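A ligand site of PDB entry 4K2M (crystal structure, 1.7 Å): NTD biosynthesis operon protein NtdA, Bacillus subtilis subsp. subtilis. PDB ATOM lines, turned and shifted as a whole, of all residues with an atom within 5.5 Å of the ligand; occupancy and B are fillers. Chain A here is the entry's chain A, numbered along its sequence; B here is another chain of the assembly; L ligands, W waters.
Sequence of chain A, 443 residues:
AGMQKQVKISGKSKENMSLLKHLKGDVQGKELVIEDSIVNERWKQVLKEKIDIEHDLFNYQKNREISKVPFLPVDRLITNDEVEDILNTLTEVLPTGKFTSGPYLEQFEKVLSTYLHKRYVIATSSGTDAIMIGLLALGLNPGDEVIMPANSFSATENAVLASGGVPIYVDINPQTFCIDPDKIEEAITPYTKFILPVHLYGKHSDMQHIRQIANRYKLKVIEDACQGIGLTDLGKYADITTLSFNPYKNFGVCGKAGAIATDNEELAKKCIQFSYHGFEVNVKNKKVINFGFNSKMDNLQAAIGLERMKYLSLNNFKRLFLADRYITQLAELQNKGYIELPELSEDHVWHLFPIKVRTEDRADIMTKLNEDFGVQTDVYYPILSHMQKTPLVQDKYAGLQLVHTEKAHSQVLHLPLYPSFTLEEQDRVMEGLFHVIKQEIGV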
ATOM      1  N   SER A 126      26.978  13.626  20.031  1.00  0.00           N
ATOM      2  CA  SER A 126      25.760  13.607  20.852  1.00  0.00           C
ATOM      3  C   SER A 126      26.050  12.931  22.177  1.00  0.00           C
ATOM      4  O   SER A 126      27.075  12.287  22.332  1.00  0.00           O
ATOM      5  CB  SER A 126      24.618  12.853  20.169  1.00  0.00           C
ATOM      6  OG  SER A 126      24.892  11.459  20.091  1.00  0.00           O
ATOM      7  N   GLY A 127      25.115  13.052  23.116  1.00  0.00           N
ATOM      8  CA  GLY A 127      25.198  12.355  24.392  1.00  0.00           C
ATOM      9  C   GLY A 127      25.100  10.861  24.189  1.00  0.00           C
ATOM     10  O   GLY A 127      25.824  10.088  24.822  1.00  0.00           O
ATOM     11  N   THR A 128      24.224  10.435  23.276  1.00  0.00           N
ATOM     12  CA  THR A 128      24.088   9.014  22.969  1.00  0.00           C
ATOM     13  C   THR A 128      25.421   8.424  22.506  1.00  0.00           C
ATOM     14  O   THR A 128      25.833   7.333  22.953  1.00  0.00           O
ATOM     15  CB  THR A 128      23.025   8.784  21.863  1.00  0.00           C
ATOM     16  OG1 THR A 128      21.762   9.298  22.313  1.00  0.00           O
ATOM     17  CG2 THR A 128      22.873   7.291  21.559  1.00  0.00           C
ATOM     18  N   ASP A 129      26.092   9.155  21.626  1.00  0.00           N
ATOM     19  CA  ASP A 129      27.387   8.711  21.113  1.00  0.00           C
ATOM     20  C   ASP A 129      28.433   8.678  22.222  1.00  0.00           C
ATOM     21  O   ASP A 129      29.278   7.792  22.251  1.00  0.00           O
ATOM     22  CB  ASP A 129      27.861   9.625  19.969  1.00  0.00           C
ATOM     23  CG  ASP A 129      26.994   9.498  18.721  1.00  0.00           C
ATOM     24  OD1 ASP A 129      27.001   8.400  18.117  1.00  0.00           O
ATOM     25  OD2 ASP A 129      26.320  10.487  18.341  1.00  0.00           O
ATOM     26  N   ILE A 131      27.923   7.928  25.359  1.00  0.00           N
ATOM     27  CA  ILE A 131      27.750   6.696  26.133  1.00  0.00           C
ATOM     28  C   ILE A 131      28.248   5.496  25.345  1.00  0.00           C
ATOM     29  O   ILE A 131      28.950   4.626  25.880  1.00  0.00           O
ATOM     30  CB  ILE A 131      26.283   6.508  26.545  1.00  0.00           C
ATOM     31  CG1 ILE A 131      25.828   7.704  27.385  1.00  0.00           C
ATOM     32  CG2 ILE A 131      26.116   5.165  27.310  1.00  0.00           C
ATOM     33  CD1 ILE A 131      24.296   7.811  27.527  1.00  0.00           C
ATOM     34  N   SER A 152      15.085   5.903  32.180  1.00  0.00           N
ATOM     35  CA  SER A 152      15.792   6.986  31.504  1.00  0.00           C
ATOM     36  C   SER A 152      15.180   7.219  30.119  1.00  0.00           C
ATOM     37  O   SER A 152      14.287   6.498  29.681  1.00  0.00           O
ATOM     38  CB  SER A 152      17.283   6.625  31.365  1.00  0.00           C
ATOM     39  OG  SER A 152      18.013   7.738  30.875  1.00  0.00           O
ATOM     40  N   PHE A 153      15.671   8.242  29.422  1.00  0.00           N
ATOM     41  CA  PHE A 153      15.327   8.428  28.016  1.00  0.00           C
ATOM     42  C   PHE A 153      15.897   7.234  27.239  1.00  0.00           C
ATOM     43  O   PHE A 153      16.901   6.648  27.647  1.00  0.00           O
ATOM     44  CB  PHE A 153      15.953   9.743  27.535  1.00  0.00           C
ATOM     45  CG  PHE A 153      15.700  10.045  26.072  1.00  0.00           C
ATOM     46  CD1 PHE A 153      14.398  10.159  25.582  1.00  0.00           C
ATOM     47  CD2 PHE A 153      16.762  10.240  25.213  1.00  0.00           C
ATOM     48  CE1 PHE A 153      14.173  10.448  24.230  1.00  0.00           C
ATOM     49  CE2 PHE A 153      16.543  10.509  23.853  1.00  0.00           C
ATOM     50  CZ  PHE A 153      15.250  10.624  23.368  1.00  0.00           C
ATOM     51  N   ALA A 155      17.705   6.807  24.906  1.00  0.00           N
ATOM     52  CA  ALA A 155      19.093   6.906  24.447  1.00  0.00           C
ATOM     53  C   ALA A 155      20.064   6.082  25.279  1.00  0.00           C
ATOM     54  O   ALA A 155      21.042   5.558  24.754  1.00  0.00           O
ATOM     55  CB  ALA A 155      19.538   8.365  24.477  1.00  0.00           C
ATOM     56  N   THR A 156      19.785   5.976  26.579  1.00  0.00           N
ATOM     57  CA  THR A 156      20.710   5.291  27.478  1.00  0.00           C
ATOM     58  C   THR A 156      20.773   3.805  27.086  1.00  0.00           C
ATOM     59  O   THR A 156      21.863   3.261  26.831  1.00  0.00           O
ATOM     60  CB  THR A 156      20.309   5.472  28.955  1.00  0.00           C
ATOM     61  OG1 THR A 156      20.043   6.855  29.234  1.00  0.00           O
ATOM     62  CG2 THR A 156      21.417   4.966  29.893  1.00  0.00           C
ATOM     63  N   VAL A 198      22.135   6.794  35.985  1.00  0.00           N
ATOM     64  CA  VAL A 198      21.666   7.990  35.294  1.00  0.00           C
ATOM     65  C   VAL A 198      21.311   9.062  36.310  1.00  0.00           C
ATOM     66  O   VAL A 198      20.567   8.810  37.257  1.00  0.00           O
ATOM     67  CB  VAL A 198      20.437   7.685  34.452  1.00  0.00           C
ATOM     68  CG1 VAL A 198      19.965   8.950  33.704  1.00  0.00           C
ATOM     69  CG2 VAL A 198      20.729   6.548  33.472  1.00  0.00           C
ATOM     70  N   LEU A 200      19.081  11.256  36.713  1.00  0.00           N
ATOM     71  CA  LEU A 200      17.831  11.558  36.039  1.00  0.00           C
ATOM     72  C   LEU A 200      17.190  12.826  36.565  1.00  0.00           C
ATOM     73  O   LEU A 200      17.143  13.059  37.784  1.00  0.00           O
ATOM     74  CB  LEU A 200      16.855  10.401  36.231  1.00  0.00           C
ATOM     75  CG  LEU A 200      15.634  10.425  35.316  1.00  0.00           C
ATOM     76  CD1 LEU A 200      16.045  10.425  33.823  1.00  0.00           C
ATOM     77  CD2 LEU A 200      14.767   9.202  35.624  1.00  0.00           C
ATOM     78  N   ASP A 224      25.703   8.368  33.180  1.00  0.00           N
ATOM     79  CA  ASP A 224      24.982   9.149  32.198  1.00  0.00           C
ATOM     80  C   ASP A 224      24.601  10.418  32.929  1.00  0.00           C
ATOM     81  O   ASP A 224      23.636  10.450  33.689  1.00  0.00           O
ATOM     82  CB  ASP A 224      23.724   8.404  31.769  1.00  0.00           C
ATOM     83  CG  ASP A 224      22.873   9.173  30.783  1.00  0.00           C
ATOM     84  OD1 ASP A 224      23.054  10.400  30.649  1.00  0.00           O
ATOM     85  OD2 ASP A 224      22.005   8.548  30.170  1.00  0.00           O
ATOM     86  N   CYS A 226      23.946  13.147  31.236  1.00  0.00           N
ATOM     87  CA  CYS A 226      23.479  13.997  30.138  1.00  0.00           C
ATOM     88  C   CYS A 226      22.520  15.112  30.575  1.00  0.00           C
ATOM     89  O   CYS A 226      22.461  16.177  29.936  1.00  0.00           O
ATOM     90  CB  CYS A 226      22.905  13.157  28.998  1.00  0.00           C
ATOM     91  SG  CYS A 226      24.201  12.208  28.144  1.00  0.00           S
ATOM     92  N   GLN A 227      21.816  14.900  31.693  1.00  0.00           N
ATOM     93  CA  GLN A 227      20.919  15.934  32.234  1.00  0.00           C
ATOM     94  C   GLN A 227      21.486  16.626  33.470  1.00  0.00           C
ATOM     95  O   GLN A 227      20.785  17.382  34.132  1.00  0.00           O
ATOM     96  CB  GLN A 227      19.570  15.313  32.610  1.00  0.00           C
ATOM     97  CG  GLN A 227      18.746  14.869  31.392  1.00  0.00           C
ATOM     98  CD  GLN A 227      17.421  14.241  31.790  1.00  0.00           C
ATOM     99  OE1 GLN A 227      17.026  14.269  32.950  1.00  0.00           O
ATOM    100  NE2 GLN A 227      16.724  13.657  30.814  1.00  0.00           N
ATOM    101  N   SER A 244      25.426  15.574  27.577  1.00  0.00           N
ATOM    102  CA  SER A 244      24.746  15.977  26.349  1.00  0.00           C
ATOM    103  C   SER A 244      24.698  17.487  26.287  1.00  0.00           C
ATOM    104  O   SER A 244      24.507  18.133  27.333  1.00  0.00           O
ATOM    105  CB  SER A 244      23.297  15.492  26.329  1.00  0.00           C
ATOM    106  OG  SER A 244      22.616  16.060  25.210  1.00  0.00           O
ATOM    107  N   PHE A 245      24.879  18.041  25.097  1.00  0.00           N
ATOM    108  CA  PHE A 245      24.713  19.484  24.873  1.00  0.00           C
ATOM    109  C   PHE A 245      23.597  19.696  23.875  1.00  0.00           C
ATOM    110  O   PHE A 245      23.579  20.660  23.123  1.00  0.00           O
ATOM    111  CB  PHE A 245      26.015  20.116  24.355  1.00  0.00           C
ATOM    112  CG  PHE A 245      27.199  19.825  25.219  1.00  0.00           C
ATOM    113  CD1 PHE A 245      27.160  20.085  26.585  1.00  0.00           C
ATOM    114  CD2 PHE A 245      28.331  19.245  24.686  1.00  0.00           C
ATOM    115  CE1 PHE A 245      28.248  19.794  27.394  1.00  0.00           C
ATOM    116  CE2 PHE A 245      29.427  18.953  25.478  1.00  0.00           C
ATOM    117  CZ  PHE A 245      29.391  19.223  26.834  1.00  0.00           C
ATOM    118  N   ASN A 246      22.637  18.774  23.877  1.00  0.00           N
ATOM    119  CA  ASN A 246      21.416  18.975  23.117  1.00  0.00           C
ATOM    120  C   ASN A 246      20.777  20.320  23.546  1.00  0.00           C
ATOM    121  O   ASN A 246      20.921  20.750  24.709  1.00  0.00           O
ATOM    122  CB  ASN A 246      20.495  17.764  23.345  1.00  0.00           C
ATOM    123  CG  ASN A 246      19.043  18.053  23.073  1.00  0.00           C
ATOM    124  OD1 ASN A 246      18.338  18.585  23.941  1.00  0.00           O
ATOM    125  ND2 ASN A 246      18.552  17.671  21.884  1.00  0.00           N
ATOM    126  N   PRO A 247      20.116  21.018  22.623  1.00  0.00           N
ATOM    127  CA  PRO A 247      19.622  22.362  22.952  1.00  0.00           C
ATOM    128  C   PRO A 247      18.631  22.456  24.096  1.00  0.00           C
ATOM    129  O   PRO A 247      18.405  23.579  24.567  1.00  0.00           O
ATOM    130  CB  PRO A 247      18.929  22.781  21.652  1.00  0.00           C
ATOM    131  CG  PRO A 247      19.653  22.043  20.595  1.00  0.00           C
ATOM    132  CD  PRO A 247      19.960  20.697  21.191  1.00  0.00           C
ATOM    133  N   TYR A 248      18.009  21.360  24.514  1.00  0.00           N
ATOM    134  CA  TYR A 248      17.083  21.430  25.642  1.00  0.00           C
ATOM    135  C   TYR A 248      17.772  21.212  26.974  1.00  0.00           C
ATOM    136  O   TYR A 248      17.132  21.315  28.024  1.00  0.00           O
ATOM    137  CB  TYR A 248      15.946  20.416  25.499  1.00  0.00           C
ATOM    138  CG  TYR A 248      15.414  20.293  24.095  1.00  0.00           C
ATOM    139  CD1 TYR A 248      15.160  21.416  23.313  1.00  0.00           C
ATOM    140  CD2 TYR A 248      15.180  19.045  23.546  1.00  0.00           C
ATOM    141  CE1 TYR A 248      14.683  21.282  22.011  1.00  0.00           C
ATOM    142  CE2 TYR A 248      14.701  18.902  22.275  1.00  0.00           C
ATOM    143  CZ  TYR A 248      14.441  20.005  21.513  1.00  0.00           C
ATOM    144  OH  TYR A 248      13.972  19.832  20.226  1.00  0.00           O
ATOM    145  N   LYS A 249      19.067  20.908  26.966  1.00  0.00           N
ATOM    146  CA  LYS A 249      19.773  20.619  28.229  1.00  0.00           C
ATOM    147  C   LYS A 249      20.075  21.913  29.005  1.00  0.00           C
ATOM    148  O   LYS A 249      19.932  23.026  28.494  1.00  0.00           O
ATOM    149  CB  LYS A 249      21.057  19.812  27.973  1.00  0.00           C
ATOM    150  CG  LYS A 249      20.839  18.440  27.299  1.00  0.00           C
ATOM    151  CD  LYS A 249      19.933  17.535  28.128  1.00  0.00           C
ATOM    152  CE  LYS A 249      19.572  16.295  27.324  1.00  0.00           C
ATOM    153  NZ  LYS A 249      18.621  16.668  26.215  1.00  0.00           N
ATOM    154  N   ALA A 257      25.322  17.480  20.182  1.00  0.00           N
ATOM    155  CA  ALA A 257      26.695  17.373  20.660  1.00  0.00           C
ATOM    156  C   ALA A 257      26.676  16.751  22.044  1.00  0.00           C
ATOM    157  O   ALA A 257      25.639  16.742  22.705  1.00  0.00           O
ATOM    158  CB  ALA A 257      27.362  18.762  20.702  1.00  0.00           C
ATOM    159  N   HIS A 351      17.084  19.948  35.966  1.00  0.00           N
ATOM    160  CA  HIS A 351      16.805  19.908  34.545  1.00  0.00           C
ATOM    161  C   HIS A 351      15.292  19.730  34.299  1.00  0.00           C
ATOM    162  O   HIS A 351      14.709  20.366  33.412  1.00  0.00           O
ATOM    163  CB  HIS A 351      17.551  18.755  33.880  1.00  0.00           C
ATOM    164  CG  HIS A 351      17.222  18.608  32.425  1.00  0.00           C
ATOM    165  ND1 HIS A 351      17.514  19.584  31.495  1.00  0.00           N
ATOM    166  CD2 HIS A 351      16.596  17.611  31.755  1.00  0.00           C
ATOM    167  CE1 HIS A 351      17.092  19.188  30.305  1.00  0.00           C
ATOM    168  NE2 HIS A 351      16.534  18.007  30.433  1.00  0.00           N
ATOM    169  N   LEU A 352      14.680  18.840  35.085  1.00  0.00           N
ATOM    170  CA  LEU A 352      13.234  18.638  35.088  1.00  0.00           C
ATOM    171  C   LEU A 352      12.784  18.693  36.532  1.00  0.00           C
ATOM    172  O   LEU A 352      13.581  18.439  37.440  1.00  0.00           O
ATOM    173  CB  LEU A 352      12.869  17.293  34.437  1.00  0.00           C
ATOM    174  CG  LEU A 352      13.058  17.292  32.898  1.00  0.00           C
ATOM    175  CD1 LEU A 352      13.420  15.906  32.334  1.00  0.00           C
ATOM    176  CD2 LEU A 352      11.819  17.855  32.186  1.00  0.00           C
ATOM    177  N   TYR A 380       8.158  12.757  31.679  1.00  0.00           N
ATOM    178  CA  TYR A 380       9.394  12.235  31.095  1.00  0.00           C
ATOM    179  C   TYR A 380       9.756  10.961  31.870  1.00  0.00           C
ATOM    180  O   TYR A 380      10.180  11.065  33.028  1.00  0.00           O
ATOM    181  CB  TYR A 380      10.531  13.270  31.261  1.00  0.00           C
ATOM    182  CG  TYR A 380      10.475  14.464  30.317  1.00  0.00           C
ATOM    183  CD1 TYR A 380       9.377  15.318  30.295  1.00  0.00           C
ATOM    184  CD2 TYR A 380      11.557  14.752  29.490  1.00  0.00           C
ATOM    185  CE1 TYR A 380       9.338  16.406  29.413  1.00  0.00           C
ATOM    186  CE2 TYR A 380      11.540  15.853  28.630  1.00  0.00           C
ATOM    187  CZ  TYR A 380      10.427  16.675  28.600  1.00  0.00           C
ATOM    188  OH  TYR A 380      10.402  17.755  27.736  1.00  0.00           O
ATOM    189  N   TYR A 381       9.623   9.771  31.280  1.00  0.00           N
ATOM    190  CA  TYR A 381       9.267   9.504  29.889  1.00  0.00           C
ATOM    191  C   TYR A 381       8.068   8.551  29.915  1.00  0.00           C
ATOM    192  O   TYR A 381       7.807   7.924  30.936  1.00  0.00           O
ATOM    193  CB  TYR A 381      10.471   8.872  29.158  1.00  0.00           C
ATOM    194  CG  TYR A 381      11.619   9.852  29.164  1.00  0.00           C
ATOM    195  CD1 TYR A 381      11.750  10.790  28.162  1.00  0.00           C
ATOM    196  CD2 TYR A 381      12.527   9.885  30.222  1.00  0.00           C
ATOM    197  CE1 TYR A 381      12.785  11.739  28.182  1.00  0.00           C
ATOM    198  CE2 TYR A 381      13.562  10.835  30.265  1.00  0.00           C
ATOM    199  CZ  TYR A 381      13.676  11.750  29.233  1.00  0.00           C
ATOM    200  OH  TYR A 381      14.689  12.688  29.255  1.00  0.00           O
ATOM    201  N   THR B 100      17.669  20.894  16.336  1.00  0.00           N
ATOM    202  CA  THR B 100      17.769  19.456  16.070  1.00  0.00           C
ATOM    203  C   THR B 100      16.534  19.031  15.269  1.00  0.00           C
ATOM    204  O   THR B 100      16.593  18.919  14.044  1.00  0.00           O
ATOM    205  CB  THR B 100      17.924  18.666  17.378  1.00  0.00           C
ATOM    206  OG1 THR B 100      16.905  19.071  18.290  1.00  0.00           O
ATOM    207  CG2 THR B 100      19.283  18.985  18.004  1.00  0.00           C
ATOM    208  N   SER B 101      15.419  18.794  15.938  1.00  0.00           N
ATOM    209  CA  SER B 101      14.158  18.602  15.236  1.00  0.00           C
ATOM    210  C   SER B 101      13.692  19.945  14.699  1.00  0.00           C
ATOM    211  O   SER B 101      13.929  20.986  15.315  1.00  0.00           O
ATOM    212  CB  SER B 101      13.102  18.029  16.172  1.00  0.00           C
ATOM    213  OG  SER B 101      13.000  18.799  17.357  1.00  0.00           O
ATOM    214  N   TYR B 276      16.536   7.267  14.556  1.00  0.00           N
ATOM    215  CA  TYR B 276      16.059   8.001  15.703  1.00  0.00           C
ATOM    216  C   TYR B 276      15.543   7.081  16.795  1.00  0.00           C
ATOM    217  O   TYR B 276      14.339   6.980  17.019  1.00  0.00           O
ATOM    218  CB  TYR B 276      14.965   8.980  15.277  1.00  0.00           C
ATOM    219  CG  TYR B 276      14.687  10.039  16.296  1.00  0.00           C
ATOM    220  CD1 TYR B 276      15.711  10.826  16.816  1.00  0.00           C
ATOM    221  CD2 TYR B 276      13.390  10.269  16.741  1.00  0.00           C
ATOM    222  CE1 TYR B 276      15.453  11.823  17.756  1.00  0.00           C
ATOM    223  CE2 TYR B 276      13.119  11.265  17.686  1.00  0.00           C
ATOM    224  CZ  TYR B 276      14.159  12.023  18.180  1.00  0.00           C
ATOM    225  OH  TYR B 276      13.906  13.010  19.112  1.00  0.00           O
ATOM    226  N   HIS B 277      16.484   6.419  17.460  1.00  0.00           N
ATOM    227  CA  HIS B 277      16.243   5.733  18.743  1.00  0.00           C
ATOM    228  C   HIS B 277      15.351   4.513  18.666  1.00  0.00           C
ATOM    229  O   HIS B 277      14.982   3.936  19.693  1.00  0.00           O
ATOM    230  CB  HIS B 277      15.704   6.709  19.797  1.00  0.00           C
ATOM    231  CG  HIS B 277      16.715   7.742  20.213  1.00  0.00           C
ATOM    232  ND1 HIS B 277      17.878   7.412  20.892  1.00  0.00           N
ATOM    233  CD2 HIS B 277      16.754   9.075  20.026  1.00  0.00           C
ATOM    234  CE1 HIS B 277      18.579   8.509  21.102  1.00  0.00           C
ATOM    235  NE2 HIS B 277      17.918   9.534  20.587  1.00  0.00           N
ATOM    236  N   LYS B 284       7.613  10.011  19.309  1.00  0.00           N
ATOM    237  CA  LYS B 284       8.780  10.010  20.166  1.00  0.00           C
ATOM    238  C   LYS B 284       8.535   9.140  21.380  1.00  0.00           C
ATOM    239  O   LYS B 284       7.412   9.067  21.882  1.00  0.00           O
ATOM    240  CB  LYS B 284       9.075  11.441  20.610  1.00  0.00           C
ATOM    241  CG  LYS B 284      10.452  11.629  21.201  1.00  0.00           C
ATOM    242  CD  LYS B 284      10.622  13.088  21.622  1.00  0.00           C
ATOM    243  CE  LYS B 284      12.053  13.367  22.072  1.00  0.00           C
ATOM    244  NZ  LYS B 284      12.290  14.852  22.239  1.00  0.00           N
ATOM    245  N   ASN B 294      21.006   8.081  17.523  1.00  0.00           N
ATOM    246  CA  ASN B 294      20.597   9.469  17.485  1.00  0.00           C
ATOM    247  C   ASN B 294      21.274  10.087  16.278  1.00  0.00           C
ATOM    248  O   ASN B 294      22.281  10.786  16.395  1.00  0.00           O
ATOM    249  CB  ASN B 294      20.992  10.168  18.785  1.00  0.00           C
ATOM    250  CG  ASN B 294      20.545  11.605  18.817  1.00  0.00           C
ATOM    251  OD1 ASN B 294      19.676  12.029  18.052  1.00  0.00           O
ATOM    252  ND2 ASN B 294      21.137  12.388  19.735  1.00  0.00           N
HETATM  253  P1  LIG L   1      21.613  13.219  23.234  1.00  0.00           P
HETATM  254  C1  LIG L   1      19.025  12.012  28.294  1.00  0.00           C
HETATM  255  O1  LIG L   1      17.994  12.779  28.730  1.00  0.00           O
HETATM  256  C2  LIG L   1      14.214  14.634  25.061  1.00  0.00           C
HETATM  257  N1  LIG L   1      20.684  10.369  28.655  1.00  0.00           N
HETATM  258  C3  LIG L   1      15.257  13.980  25.959  1.00  0.00           C
HETATM  259  O2  LIG L   1      14.897  14.441  27.301  1.00  0.00           O
HETATM  260  C4  LIG L   1      19.671  11.098  29.132  1.00  0.00           C
HETATM  261  C5  LIG L   1      19.285  10.908  30.592  1.00  0.00           C
HETATM  262  C6  LIG L   1      16.699  14.369  25.603  1.00  0.00           C
HETATM  263  N2  LIG L   1      17.538  13.441  26.386  1.00  0.00           N
HETATM  264  O3  LIG L   1      14.089  16.039  25.316  1.00  0.00           O
HETATM  265  C7  LIG L   1      16.963  14.295  24.087  1.00  0.00           C
HETATM  266  O4  LIG L   1      18.147  15.121  23.955  1.00  0.00           O
HETATM  267  C8  LIG L   1      19.417  12.158  26.979  1.00  0.00           C
HETATM  268  C9  LIG L   1      18.725  13.095  26.065  1.00  0.00           C
HETATM  269  C10 LIG L   1      15.851  15.050  23.366  1.00  0.00           C
HETATM  270  O5  LIG L   1      14.566  14.492  23.683  1.00  0.00           O
HETATM  271  C11 LIG L   1      20.469  11.381  26.498  1.00  0.00           C
HETATM  272  C12 LIG L   1      21.034  11.398  25.074  1.00  0.00           C
HETATM  273  C13 LIG L   1      15.872  14.884  21.872  1.00  0.00           C
HETATM  274  C14 LIG L   1      21.079  10.486  27.364  1.00  0.00           C
HETATM  275  O6  LIG L   1      22.062  12.014  22.435  1.00  0.00           O
HETATM  276  O7  LIG L   1      22.621  14.317  23.254  1.00  0.00           O
HETATM  277  O8  LIG L   1      20.164  13.636  22.876  1.00  0.00           O
HETATM  278  O9  LIG L   1      21.584  12.704  24.789  1.00  0.00           O
HETATM  279  O10 LIG L   1      15.035  15.735  21.177  1.00  0.00           O
HETATM  280  P2  LIG L   1      15.457  16.280  19.724  1.00  0.00           P
HETATM  281  O11 LIG L   1      16.718  17.097  19.934  1.00  0.00           O
HETATM  282  O12 LIG L   1      15.628  15.105  18.799  1.00  0.00           O
HETATM  283  O13 LIG L   1      14.240  17.150  19.351  1.00  0.00           O
HETATM  284  O   HOH W   1      18.181  14.116  19.171  1.00  0.00           O
HETATM  285  O   HOH W   2      22.865  16.062  21.273  1.00  0.00           O
HETATM  286  O   HOH W   3      13.750  18.386  27.573  1.00  0.00           O
HETATM  287  O   HOH W   4      15.873  16.808  28.013  1.00  0.00           O
HETATM  288  O   HOH W   5      11.716  16.292  20.018  1.00  0.00           O
HETATM  289  O   HOH W   6      11.194  17.762  25.010  1.00  0.00           O
HETATM  290  O   HOH W   7      18.401  12.126  21.504  1.00  0.00           O
HETATM  291  O   HOH W   8      17.211  14.829  16.221  1.00  0.00           O
HETATM  292  O   HOH W   9      20.021  15.231  20.786  1.00  0.00           O
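Ser 126 touches the ligand (CB to O6, 3.5 Å).
OG of Ser 152 touches C5 of the ligand (3.4 Å).
Phe 153 touches the ligand.
Ala 155 touches the ligand (CB to C12, 3.4 Å).
Thr 156 touches the ligand (OG1 to N1, 3.6 Å).
Val 198 touches the ligand.
CB of Cys 226 touches N1 of the ligand, 3.6 Å away.
Ala 257 touches the ligand.
Tyr 380 touches the ligand (CE2 to O2, 3.9 Å).
23 residues have an atom within 4 Å of the ligand: Ser 126, Gly 127, Thr 128, Ser 152, Phe 153, Ala 155, Thr 156, Val 198, Asp 224, Cys 226, Gln 227, Ser 244, Asn 246, Tyr 248, Lys 249, Ala 257, Tyr 380, Tyr 381, Thr 100 of chain B, Ser 101 of chain B, Tyr 276 of chain B, Lys 284 of chain B and Asn 294 of chain B.
The nearest printed residue that does not touch the ligand is Ile 131 (4.2 Å).
The side-chain sulfur (SG) of Cys 226 lies close to the backbone NH (N) of Ser 244, at 3.6 Å.
OD2 of Asp 224 lies within hydrogen-bond range of OG1 of Thr 156 (2.8 Å).
The side-chain amide oxygen (OD1) of Asn 246 sits at hydrogen-bond distance from the side-chain amino group (NZ) of Lys 249, at 3.0 Å.
The backbone NH of Tyr 248 is in hydrogen-bond range of the side-chain amide oxygen of Asn 246 (2.9 Å).
The side-chain hydroxyl of Tyr 248 sits at hydrogen-bond distance from the side-chain hydroxyl of Ser 101 of chain B (3.2 Å).
OG1 of Thr 156 is in hydrogen-bond range of OG of Ser 152 (2.8 Å).
The side-chain carboxylate of Asp 129 sits at hydrogen-bond distance from the side-chain hydroxyl of Ser 126 (2.5 Å).
O of Ala 257 is in hydrogen-bond range of N of Phe 245, 2.8 Å away.
Water W2 bridges O7 of the ligand (2.7 Å) and N of Ala 257 (3.0 Å).
Water W4 lies within hydrogen-bond range of an oxygen (O2) of the ligand (2.7 Å), a ring nitrogen (NE2) of His 351 (2.8 Å) and the side-chain amino group of Lys 249 (3.3 Å).
Water W7 lies within hydrogen-bond range of an oxygen (O8) of the ligand (2.7 Å), a ring nitrogen (NE2) of His 277 of chain B (2.8 Å) and the side-chain amide nitrogen of Asn 294 of chain B (3.3 Å).
Water W5 bridges NZ of Lys 284 of chain B (2.7 Å) and O13 of the ligand (2.7 Å).
Water W3 bridges an oxygen (O3) of the ligand (3.3 Å) and the side-chain hydroxyl of Tyr 380 (3.4 Å).
Water W6 lies within hydrogen-bond range of the side-chain hydroxyl of Tyr 380 (2.8 Å) and an oxygen (O3) of the ligand (3.4 Å).
OG1 of Thr 100 of chain B is in hydrogen-bond range of O11 of the ligand, at 2.6 Å.
The side-chain amide nitrogen (NE2) of Gln 227 is in hydrogen-bond range of an oxygen (O1) of the ligand, at 2.6 Å.
O7 of the ligand sits at hydrogen-bond distance from OG of Ser 244, at 2.6 Å.
OH of Tyr 381 is in hydrogen-bond range of O2 of the ligand (2.6 Å).
N1 of the ligand is in hydrogen-bond range of OD2 of Asp 224 (2.7 Å).
An oxygen (O5) of the ligand lies within hydrogen-bond range of the side-chain amino group of Lys 284 of chain B, at 2.7 Å.
The side-chain hydroxyl (OH) of Tyr 276 of chain B sits at hydrogen-bond distance from an oxygen (O12) of the ligand (2.7 Å).
N of Thr 128 lies within hydrogen-bond range of O6 of the ligand, at 2.8 Å.
An oxygen (O6) of the ligand is in hydrogen-bond range of the side-chain hydroxyl (OG1) of Thr 128 (2.7 Å).
The side-chain amide nitrogen (ND2) of Asn 246 lies within hydrogen-bond range of an oxygen (O11) of the ligand (2.7 Å).
The side-chain amino group (NZ) of Lys 249 sits at hydrogen-bond distance from an oxygen (O4) of the ligand (2.8 Å).
An oxygen (O7) of the ligand sits at hydrogen-bond distance from the backbone NH (N) of Gly 127 (2.8 Å).
The side-chain hydroxyl of Tyr 248 sits at hydrogen-bond distance from an oxygen (O13) of the ligand (2.8 Å).
An oxygen (O13) of the ligand lies within hydrogen-bond range of the side-chain hydroxyl (OG) of Ser 101 of chain B (2.9 Å).
The side-chain amide nitrogen of Asn 294 of chain B sits at hydrogen-bond distance from an oxygen (O6) of the ligand.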
